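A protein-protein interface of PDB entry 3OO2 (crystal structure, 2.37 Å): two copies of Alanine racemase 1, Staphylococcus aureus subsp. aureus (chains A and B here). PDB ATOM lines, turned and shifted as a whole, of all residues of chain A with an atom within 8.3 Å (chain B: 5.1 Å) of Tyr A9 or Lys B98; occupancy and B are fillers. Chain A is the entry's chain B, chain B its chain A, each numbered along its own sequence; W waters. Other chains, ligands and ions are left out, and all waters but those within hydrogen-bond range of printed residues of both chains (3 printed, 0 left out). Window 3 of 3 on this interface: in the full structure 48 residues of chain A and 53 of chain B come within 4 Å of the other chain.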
ATOM      1  N   ASP A   6     -35.097  28.981  -3.950  1.00  0.00           N
ATOM      2  CA  ASP A   6     -33.895  28.683  -4.727  1.00  0.00           C
ATOM      3  C   ASP A   6     -34.070  28.935  -6.216  1.00  0.00           C
ATOM      4  O   ASP A   6     -35.194  28.896  -6.744  1.00  0.00           O
ATOM      5  CB  ASP A   6     -33.559  27.192  -4.596  1.00  0.00           C
ATOM      6  CG  ASP A   6     -33.060  26.801  -3.230  1.00  0.00           C
ATOM      7  OD1 ASP A   6     -32.275  27.556  -2.605  1.00  0.00           O
ATOM      8  OD2 ASP A   6     -33.393  25.681  -2.820  1.00  0.00           O
ATOM      9  N   LYS A   7     -32.946  29.173  -6.892  1.00  0.00           N
ATOM     10  CA  LYS A   7     -32.917  29.290  -8.340  1.00  0.00           C
ATOM     11  C   LYS A   7     -32.764  27.873  -8.911  1.00  0.00           C
ATOM     12  O   LYS A   7     -32.563  26.921  -8.160  1.00  0.00           O
ATOM     13  CB  LYS A   7     -31.728  30.133  -8.811  1.00  0.00           C
ATOM     14  CG  LYS A   7     -31.956  31.636  -8.895  1.00  0.00           C
ATOM     15  CD  LYS A   7     -32.197  32.280  -7.577  1.00  0.00           C
ATOM     16  CE  LYS A   7     -32.513  33.767  -7.766  1.00  0.00           C
ATOM     17  NZ  LYS A   7     -32.767  34.443  -6.437  1.00  0.00           N
ATOM     18  N   TYR A   8     -32.909  27.734 -10.230  1.00  0.00           N
ATOM     19  CA  TYR A   8     -32.674  26.451 -10.905  1.00  0.00           C
ATOM     20  C   TYR A   8     -32.321  26.724 -12.365  1.00  0.00           C
ATOM     21  O   TYR A   8     -32.841  27.653 -12.973  1.00  0.00           O
ATOM     22  CB  TYR A   8     -33.830  25.461 -10.738  1.00  0.00           C
ATOM     23  CG  TYR A   8     -35.060  25.764 -11.530  1.00  0.00           C
ATOM     24  CD1 TYR A   8     -35.998  26.677 -11.075  1.00  0.00           C
ATOM     25  CD2 TYR A   8     -35.312  25.107 -12.723  1.00  0.00           C
ATOM     26  CE1 TYR A   8     -37.152  26.939 -11.810  1.00  0.00           C
ATOM     27  CE2 TYR A   8     -36.453  25.361 -13.455  1.00  0.00           C
ATOM     28  CZ  TYR A   8     -37.366  26.280 -12.999  1.00  0.00           C
ATOM     29  OH  TYR A   8     -38.502  26.515 -13.730  1.00  0.00           O
ATOM     30  N   TYR A   9     -31.432  25.925 -12.930  1.00  0.00           N
ATOM     31  CA  TYR A   9     -30.914  26.213 -14.254  1.00  0.00           C
ATOM     32  C   TYR A   9     -31.000  25.136 -15.316  1.00  0.00           C
ATOM     33  O   TYR A   9     -30.117  25.001 -16.149  1.00  0.00           O
ATOM     34  CB  TYR A   9     -29.488  26.627 -14.084  1.00  0.00           C
ATOM     35  CG  TYR A   9     -29.373  27.803 -13.150  1.00  0.00           C
ATOM     36  CD1 TYR A   9     -29.710  29.065 -13.577  1.00  0.00           C
ATOM     37  CD2 TYR A   9     -28.939  27.648 -11.841  1.00  0.00           C
ATOM     38  CE1 TYR A   9     -29.621  30.134 -12.753  1.00  0.00           C
ATOM     39  CE2 TYR A   9     -28.830  28.732 -11.007  1.00  0.00           C
ATOM     40  CZ  TYR A   9     -29.165  29.975 -11.480  1.00  0.00           C
ATOM     41  OH  TYR A   9     -29.054  31.081 -10.686  1.00  0.00           O
ATOM     42  N   ARG A  10     -32.060  24.353 -15.269  1.00  0.00           N
ATOM     43  CA  ARG A  10     -32.306  23.369 -16.308  1.00  0.00           C
ATOM     44  C   ARG A  10     -33.806  23.294 -16.381  1.00  0.00           C
ATOM     45  O   ARG A  10     -34.491  23.245 -15.369  1.00  0.00           O
ATOM     46  CB  ARG A  10     -31.690  22.008 -15.964  1.00  0.00           C
ATOM     47  CG  ARG A  10     -31.894  20.916 -17.012  1.00  0.00           C
ATOM     48  CD  ARG A  10     -31.367  19.546 -16.526  1.00  0.00           C
ATOM     49  NE  ARG A  10     -31.984  19.120 -15.266  1.00  0.00           N
ATOM     50  CZ  ARG A  10     -32.060  17.857 -14.850  1.00  0.00           C
ATOM     51  NH1 ARG A  10     -31.584  16.864 -15.583  1.00  0.00           N
ATOM     52  NH2 ARG A  10     -32.631  17.578 -13.689  1.00  0.00           N
ATOM     53  N   SER A  11     -34.341  23.257 -17.574  1.00  0.00           N
ATOM     54  CA  SER A  11     -35.777  23.246 -17.695  1.00  0.00           C
ATOM     55  C   SER A  11     -36.384  21.868 -17.447  1.00  0.00           C
ATOM     56  O   SER A  11     -36.964  21.280 -18.334  1.00  0.00           O
ATOM     57  CB  SER A  11     -36.142  23.801 -19.067  1.00  0.00           C
ATOM     58  OG  SER A  11     -35.511  25.076 -19.221  1.00  0.00           O
ATOM     59  N   ALA A  12     -36.223  21.353 -16.234  1.00  0.00           N
ATOM     60  CA  ALA A  12     -36.791  20.038 -15.843  1.00  0.00           C
ATOM     61  C   ALA A  12     -37.087  20.162 -14.392  1.00  0.00           C
ATOM     62  O   ALA A  12     -36.236  20.580 -13.598  1.00  0.00           O
ATOM     63  CB  ALA A  12     -35.828  18.889 -16.094  1.00  0.00           C
ATOM     64  N   PRO A 284     -34.080  17.547 -21.518  1.00  0.00           N
ATOM     65  CA  PRO A 284     -33.009  17.570 -20.585  1.00  0.00           C
ATOM     66  C   PRO A 284     -33.432  16.900 -19.313  1.00  0.00           C
ATOM     67  O   PRO A 284     -33.534  17.545 -18.293  1.00  0.00           O
ATOM     68  CB  PRO A 284     -32.798  19.056 -20.356  1.00  0.00           C
ATOM     69  CG  PRO A 284     -34.175  19.632 -20.442  1.00  0.00           C
ATOM     70  CD  PRO A 284     -34.950  18.730 -21.373  1.00  0.00           C
ATOM     71  N   ARG A 366     -31.679  15.716  -8.062  1.00  0.00           N
ATOM     72  CA  ARG A 366     -31.337  16.646  -9.171  1.00  0.00           C
ATOM     73  C   ARG A 366     -32.548  17.461  -9.655  1.00  0.00           C
ATOM     74  O   ARG A 366     -32.391  18.473 -10.287  1.00  0.00           O
ATOM     75  CB  ARG A 366     -30.797  15.908 -10.397  1.00  0.00           C
ATOM     76  CG  ARG A 366     -29.619  16.614 -10.991  1.00  0.00           C
ATOM     77  CD  ARG A 366     -29.477  16.694 -12.486  1.00  0.00           C
ATOM     78  NE  ARG A 366     -29.802  15.563 -13.358  1.00  0.00           N
ATOM     79  CZ  ARG A 366     -28.947  14.861 -14.111  1.00  0.00           C
ATOM     80  NH1 ARG A 366     -29.424  13.989 -14.968  1.00  0.00           N
ATOM     81  NH2 ARG A 366     -27.644  15.073 -14.090  1.00  0.00           N
ATOM     82  N   PRO A 368     -35.635  19.978  -9.335  1.00  0.00           N
ATOM     83  CA  PRO A 368     -36.159  20.975  -8.423  1.00  0.00           C
ATOM     84  C   PRO A 368     -37.613  20.713  -8.160  1.00  0.00           C
ATOM     85  O   PRO A 368     -38.301  20.234  -9.037  1.00  0.00           O
ATOM     86  CB  PRO A 368     -36.008  22.284  -9.204  1.00  0.00           C
ATOM     87  CG  PRO A 368     -34.909  22.000 -10.211  1.00  0.00           C
ATOM     88  CD  PRO A 368     -35.217  20.586 -10.607  1.00  0.00           C
ATOM     89  N   VAL A 379     -39.409  27.439  -4.770  1.00  0.00           N
ATOM     90  CA  VAL A 379     -38.538  26.407  -5.278  1.00  0.00           C
ATOM     91  C   VAL A 379     -37.534  25.866  -4.245  1.00  0.00           C
ATOM     92  O   VAL A 379     -37.091  26.569  -3.322  1.00  0.00           O
ATOM     93  CB  VAL A 379     -37.793  26.879  -6.529  1.00  0.00           C
ATOM     94  CG1 VAL A 379     -36.933  25.743  -7.089  1.00  0.00           C
ATOM     95  CG2 VAL A 379     -38.792  27.398  -7.597  1.00  0.00           C
ATOM     96  N   ASN A 381     -34.100  23.533  -4.657  1.00  0.00           N
ATOM     97  CA  ASN A 381     -33.111  22.926  -5.558  1.00  0.00           C
ATOM     98  C   ASN A 381     -32.041  22.445  -4.614  1.00  0.00           C
ATOM     99  O   ASN A 381     -31.219  23.219  -4.162  1.00  0.00           O
ATOM    100  CB  ASN A 381     -32.563  23.945  -6.560  1.00  0.00           C
ATOM    101  CG  ASN A 381     -31.635  23.318  -7.611  1.00  0.00           C
ATOM    102  OD1 ASN A 381     -31.368  22.128  -7.589  1.00  0.00           O
ATOM    103  ND2 ASN A 381     -31.155  24.136  -8.545  1.00  0.00           N
ATOM    104  N   LEU A 384     -28.257  23.515  -4.849  1.00  0.00           N
ATOM    105  CA  LEU A 384     -27.828  24.870  -4.489  1.00  0.00           C
ATOM    106  C   LEU A 384     -28.252  25.201  -3.072  1.00  0.00           C
ATOM    107  O   LEU A 384     -28.112  26.336  -2.597  1.00  0.00           O
ATOM    108  CB  LEU A 384     -28.483  25.885  -5.410  1.00  0.00           C
ATOM    109  CG  LEU A 384     -28.352  25.651  -6.910  1.00  0.00           C
ATOM    110  CD1 LEU A 384     -29.033  26.821  -7.627  1.00  0.00           C
ATOM    111  CD2 LEU A 384     -26.888  25.499  -7.347  1.00  0.00           C
ATOM    112  N   LEU B  70     -25.815  23.467 -15.286  1.00  0.00           N
ATOM    113  CA  LEU B  70     -25.245  24.606 -14.626  1.00  0.00           C
ATOM    114  C   LEU B  70     -25.447  24.457 -13.089  1.00  0.00           C
ATOM    115  O   LEU B  70     -24.600  24.879 -12.331  1.00  0.00           O
ATOM    116  CB  LEU B  70     -25.868  25.923 -15.137  1.00  0.00           C
ATOM    117  CG  LEU B  70     -25.250  27.186 -14.512  1.00  0.00           C
ATOM    118  CD1 LEU B  70     -23.765  27.285 -14.895  1.00  0.00           C
ATOM    119  CD2 LEU B  70     -25.986  28.437 -14.913  1.00  0.00           C
ATOM    120  N   ASP B  71     -26.558  23.854 -12.635  1.00  0.00           N
ATOM    121  CA  ASP B  71     -26.771  23.698 -11.196  1.00  0.00           C
ATOM    122  C   ASP B  71     -25.612  22.884 -10.655  1.00  0.00           C
ATOM    123  O   ASP B  71     -25.047  23.195  -9.620  1.00  0.00           O
ATOM    124  CB  ASP B  71     -28.078  22.976 -10.858  1.00  0.00           C
ATOM    125  CG  ASP B  71     -29.277  23.546 -11.572  1.00  0.00           C
ATOM    126  OD1 ASP B  71     -29.993  24.366 -10.957  1.00  0.00           O
ATOM    127  OD2 ASP B  71     -29.498  23.184 -12.751  1.00  0.00           O
ATOM    128  N   ILE B  74     -22.493  25.277 -10.485  1.00  0.00           N
ATOM    129  CA  ILE B  74     -22.520  26.254  -9.410  1.00  0.00           C
ATOM    130  C   ILE B  74     -22.301  25.533  -8.061  1.00  0.00           C
ATOM    131  O   ILE B  74     -21.652  26.074  -7.188  1.00  0.00           O
ATOM    132  CB  ILE B  74     -23.821  27.094  -9.403  1.00  0.00           C
ATOM    133  CG1 ILE B  74     -23.936  27.900 -10.686  1.00  0.00           C
ATOM    134  CG2 ILE B  74     -23.825  28.068  -8.255  1.00  0.00           C
ATOM    135  CD1 ILE B  74     -25.196  28.722 -10.757  1.00  0.00           C
ATOM    136  N   LEU B  91     -27.851  25.102 -21.763  1.00  0.00           N
ATOM    137  CA  LEU B  91     -28.336  26.028 -20.740  1.00  0.00           C
ATOM    138  C   LEU B  91     -29.507  26.854 -21.288  1.00  0.00           C
ATOM    139  O   LEU B  91     -29.502  27.266 -22.452  1.00  0.00           O
ATOM    140  CB  LEU B  91     -27.204  26.981 -20.342  1.00  0.00           C
ATOM    141  CG  LEU B  91     -27.496  27.982 -19.233  1.00  0.00           C
ATOM    142  CD1 LEU B  91     -27.525  27.266 -17.927  1.00  0.00           C
ATOM    143  CD2 LEU B  91     -26.479  29.131 -19.183  1.00  0.00           C
ATOM    144  N   PRO B  92     -30.535  27.048 -20.473  1.00  0.00           N
ATOM    145  CA  PRO B  92     -31.592  27.937 -20.916  1.00  0.00           C
ATOM    146  C   PRO B  92     -30.964  29.305 -21.170  1.00  0.00           C
ATOM    147  O   PRO B  92     -30.198  29.806 -20.339  1.00  0.00           O
ATOM    148  CB  PRO B  92     -32.546  27.991 -19.724  1.00  0.00           C
ATOM    149  CG  PRO B  92     -32.309  26.773 -18.969  1.00  0.00           C
ATOM    150  CD  PRO B  92     -30.894  26.308 -19.259  1.00  0.00           C
ATOM    151  N   ASP B  95     -30.249  32.098 -18.478  1.00  0.00           N
ATOM    152  CA  ASP B  95     -29.253  31.906 -17.423  1.00  0.00           C
ATOM    153  C   ASP B  95     -27.792  32.164 -17.811  1.00  0.00           C
ATOM    154  O   ASP B  95     -26.884  31.899 -17.039  1.00  0.00           O
ATOM    155  CB  ASP B  95     -29.411  30.477 -16.914  1.00  0.00           C
ATOM    156  CG  ASP B  95     -30.854  30.159 -16.449  1.00  0.00           C
ATOM    157  OD1 ASP B  95     -31.603  31.067 -16.012  1.00  0.00           O
ATOM    158  OD2 ASP B  95     -31.218  28.978 -16.490  1.00  0.00           O
ATOM    159  N   ILE B  96     -27.577  32.704 -18.999  1.00  0.00           N
ATOM    160  CA  ILE B  96     -26.242  32.941 -19.484  1.00  0.00           C
ATOM    161  C   ILE B  96     -25.363  33.798 -18.534  1.00  0.00           C
ATOM    162  O   ILE B  96     -24.176  33.510 -18.388  1.00  0.00           O
ATOM    163  CB  ILE B  96     -26.289  33.558 -20.901  1.00  0.00           C
ATOM    164  CG1 ILE B  96     -24.969  33.284 -21.614  1.00  0.00           C
ATOM    165  CG2 ILE B  96     -26.724  35.036 -20.864  1.00  0.00           C
ATOM    166  CD1 ILE B  96     -24.750  31.797 -21.819  1.00  0.00           C
ATOM    167  N   ASP B  97     -25.941  34.819 -17.887  1.00  0.00           N
ATOM    168  CA  ASP B  97     -25.200  35.660 -16.933  1.00  0.00           C
ATOM    169  C   ASP B  97     -24.651  34.862 -15.733  1.00  0.00           C
ATOM    170  O   ASP B  97     -23.561  35.152 -15.233  1.00  0.00           O
ATOM    171  CB  ASP B  97     -26.058  36.830 -16.409  1.00  0.00           C
ATOM    172  CG  ASP B  97     -26.266  37.924 -17.428  1.00  0.00           C
ATOM    173  OD1 ASP B  97     -25.590  37.944 -18.469  1.00  0.00           O
ATOM    174  OD2 ASP B  97     -27.116  38.795 -17.179  1.00  0.00           O
ATOM    175  N   LYS B  98     -25.408  33.888 -15.248  1.00  0.00           N
ATOM    176  CA  LYS B  98     -24.926  33.067 -14.147  1.00  0.00           C
ATOM    177  C   LYS B  98     -23.747  32.178 -14.520  1.00  0.00           C
ATOM    178  O   LYS B  98     -22.958  31.824 -13.663  1.00  0.00           O
ATOM    179  CB  LYS B  98     -26.065  32.217 -13.524  1.00  0.00           C
ATOM    180  CG  LYS B  98     -26.921  33.031 -12.579  1.00  0.00           C
ATOM    181  CD  LYS B  98     -26.091  33.377 -11.347  1.00  0.00           C
ATOM    182  CE  LYS B  98     -26.622  34.581 -10.598  1.00  0.00           C
ATOM    183  NZ  LYS B  98     -27.986  34.408 -10.120  1.00  0.00           N
ATOM    184  N   ALA B  99     -23.657  31.759 -15.777  1.00  0.00           N
ATOM    185  CA  ALA B  99     -22.527  30.949 -16.198  1.00  0.00           C
ATOM    186  C   ALA B  99     -21.302  31.851 -16.236  1.00  0.00           C
ATOM    187  O   ALA B  99     -20.237  31.477 -15.761  1.00  0.00           O
ATOM    188  CB  ALA B  99     -22.774  30.310 -17.572  1.00  0.00           C
ATOM    189  N   ILE B 100     -21.479  33.055 -16.754  1.00  0.00           N
ATOM    190  CA  ILE B 100     -20.382  34.007 -16.854  1.00  0.00           C
ATOM    191  C   ILE B 100     -19.859  34.371 -15.460  1.00  0.00           C
ATOM    192  O   ILE B 100     -18.664  34.286 -15.197  1.00  0.00           O
ATOM    193  CB  ILE B 100     -20.833  35.274 -17.592  1.00  0.00           C
ATOM    194  CG1 ILE B 100     -21.333  34.911 -19.010  1.00  0.00           C
ATOM    195  CG2 ILE B 100     -19.692  36.300 -17.646  1.00  0.00           C
ATOM    196  CD1 ILE B 100     -22.038  36.072 -19.745  1.00  0.00           C
ATOM    197  N   GLN B 101     -20.779  34.781 -14.586  1.00  0.00           N
ATOM    198  CA  GLN B 101     -20.475  35.094 -13.203  1.00  0.00           C
ATOM    199  C   GLN B 101     -19.653  33.997 -12.519  1.00  0.00           C
ATOM    200  O   GLN B 101     -18.627  34.276 -11.910  1.00  0.00           O
ATOM    201  CB  GLN B 101     -21.784  35.249 -12.421  1.00  0.00           C
ATOM    202  CG  GLN B 101     -21.588  35.661 -10.953  1.00  0.00           C
ATOM    203  CD  GLN B 101     -22.880  35.540 -10.140  1.00  0.00           C
ATOM    204  OE1 GLN B 101     -23.978  35.822 -10.641  1.00  0.00           O
ATOM    205  NE2 GLN B 101     -22.750  35.112  -8.879  1.00  0.00           N
ATOM    206  N   HIS B 102     -20.132  32.748 -12.624  1.00  0.00           N
ATOM    207  CA  HIS B 102     -19.480  31.598 -11.986  1.00  0.00           C
ATOM    208  C   HIS B 102     -18.306  30.922 -12.732  1.00  0.00           C
ATOM    209  O   HIS B 102     -17.858  29.845 -12.323  1.00  0.00           O
ATOM    210  CB  HIS B 102     -20.536  30.568 -11.591  1.00  0.00           C
ATOM    211  CG  HIS B 102     -21.384  30.996 -10.437  1.00  0.00           C
ATOM    212  ND1 HIS B 102     -22.688  31.415 -10.580  1.00  0.00           N
ATOM    213  CD2 HIS B 102     -21.094  31.117  -9.120  1.00  0.00           C
ATOM    214  CE1 HIS B 102     -23.173  31.762  -9.403  1.00  0.00           C
ATOM    215  NE2 HIS B 102     -22.228  31.577  -8.497  1.00  0.00           N
HETATM  216  O   HOH W   1     -32.260  22.605 -12.288  1.00  0.00           O
HETATM  217  O   HOH W   2     -28.146  23.591 -17.282  1.00  0.00           O
HETATM  218  O   HOH W   3     -33.705  27.828 -15.679  1.00  0.00           O
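The side-chain carboxylate (OD1) of Asp B71 is in hydrogen-bond range of the side-chain amide nitrogen (ND2) of Asn A381 (2.7 Å).
The side-chain carboxylate of Asp B71 sits at hydrogen-bond distance from the backbone NH of Tyr A9 (2.9 Å).
OD2 of Asp A6 is in hydrogen-bond range of N of Asn A381 (2.9 Å).
The backbone carbonyl oxygen (O) of Lys B98 sits at hydrogen-bond distance from a ring nitrogen (ND1) of His B102 (3.1 Å).
ND2 of Asn A381 lies within hydrogen-bond range of O of Lys A7, 3.1 Å away.
The guanidinium group (NH1) of Arg A10 sits at hydrogen-bond distance from the backbone carbonyl oxygen (O) of Pro A284, at 3.4 Å.
Tyr A8 touches Asp B71.
Tyr A9 touches Leu B70.
Tyr A9 touches Ile B74 (CE2 to CD1, 3.6 Å).
Leu B91 touches Tyr A9 (CD1 to O, 3.9 Å).
Tyr A9 touches Pro B92.
Asp B95 touches Tyr A9 (CG to CD1, 3.3 Å).
Lys B98 touches Tyr A9 (CG to OH, 3.5 Å).
Arg A10 touches Asp B71.
Pro B92 touches Ser A11 (CG to OG, 3.6 Å).
Leu A384 touches Asp B71 (CD2 to O, 3.7 Å).
Tyr A9 touches just these residues of chain B: Leu B70 (3.8 Å), Asp B71 (2.9 Å), Ile B74 (3.6 Å), Leu B91 (3.9 Å), Pro B92 (3.5 Å), Asp B95 (3.3 Å) and Lys B98 (3.5 Å).
Printed residues of chain B within 4 Å of Arg A10: Asp B71.
Printed residues of chain B within 4 Å of Leu A384: Asp B71 (3.7 Å).
Printed residues of chain A within 4 Å of Leu B70: Tyr A9 (3.8 Å).
Lys B98 touches just one residue of chain A: Tyr A9 (3.5 Å).
Ile B100 touches none of the printed residues of chain A.
His B102 touches none of the printed residues of chain A.
The nearest printed residue of chain B that does not touch Tyr A9 is His B102 (6.1 Å).
The nearest residue of chain A that does not touch Lys B98 is Lys A7 (5.0 Å).
Of the 13 printed residues of chain B, 7 touch a printed residue of chain A.
Of the 13 printed residues of chain A, 6 touch a printed residue of chain B.
Hydrophobic or aromatic side chains of chain A within 4 Å of the printed part of chain B: Tyr A8, Tyr A9 and Leu A384.
No position is printed for both chains.
Of the 12 pairs that touch across the chains among the printed residues, none has its exchanged pair printed and touching as well.
Water W2 lies within hydrogen-bond range of the backbone carbonyl oxygen of Tyr A9 (2.7 Å) and the backbone NH of Leu B70 (3.1 Å).
Water W3 bridges the backbone carbonyl oxygen (O) of Tyr A8 (2.8 Å) and the side-chain carboxylate (OD2) of Asp B95 (2.9 Å).
Water W1 lies within hydrogen-bond range of OD2 of Asp B71 (2.9 Å), N of Arg A10 (3.5 Å) and N of Tyr A9 (3.5 Å).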
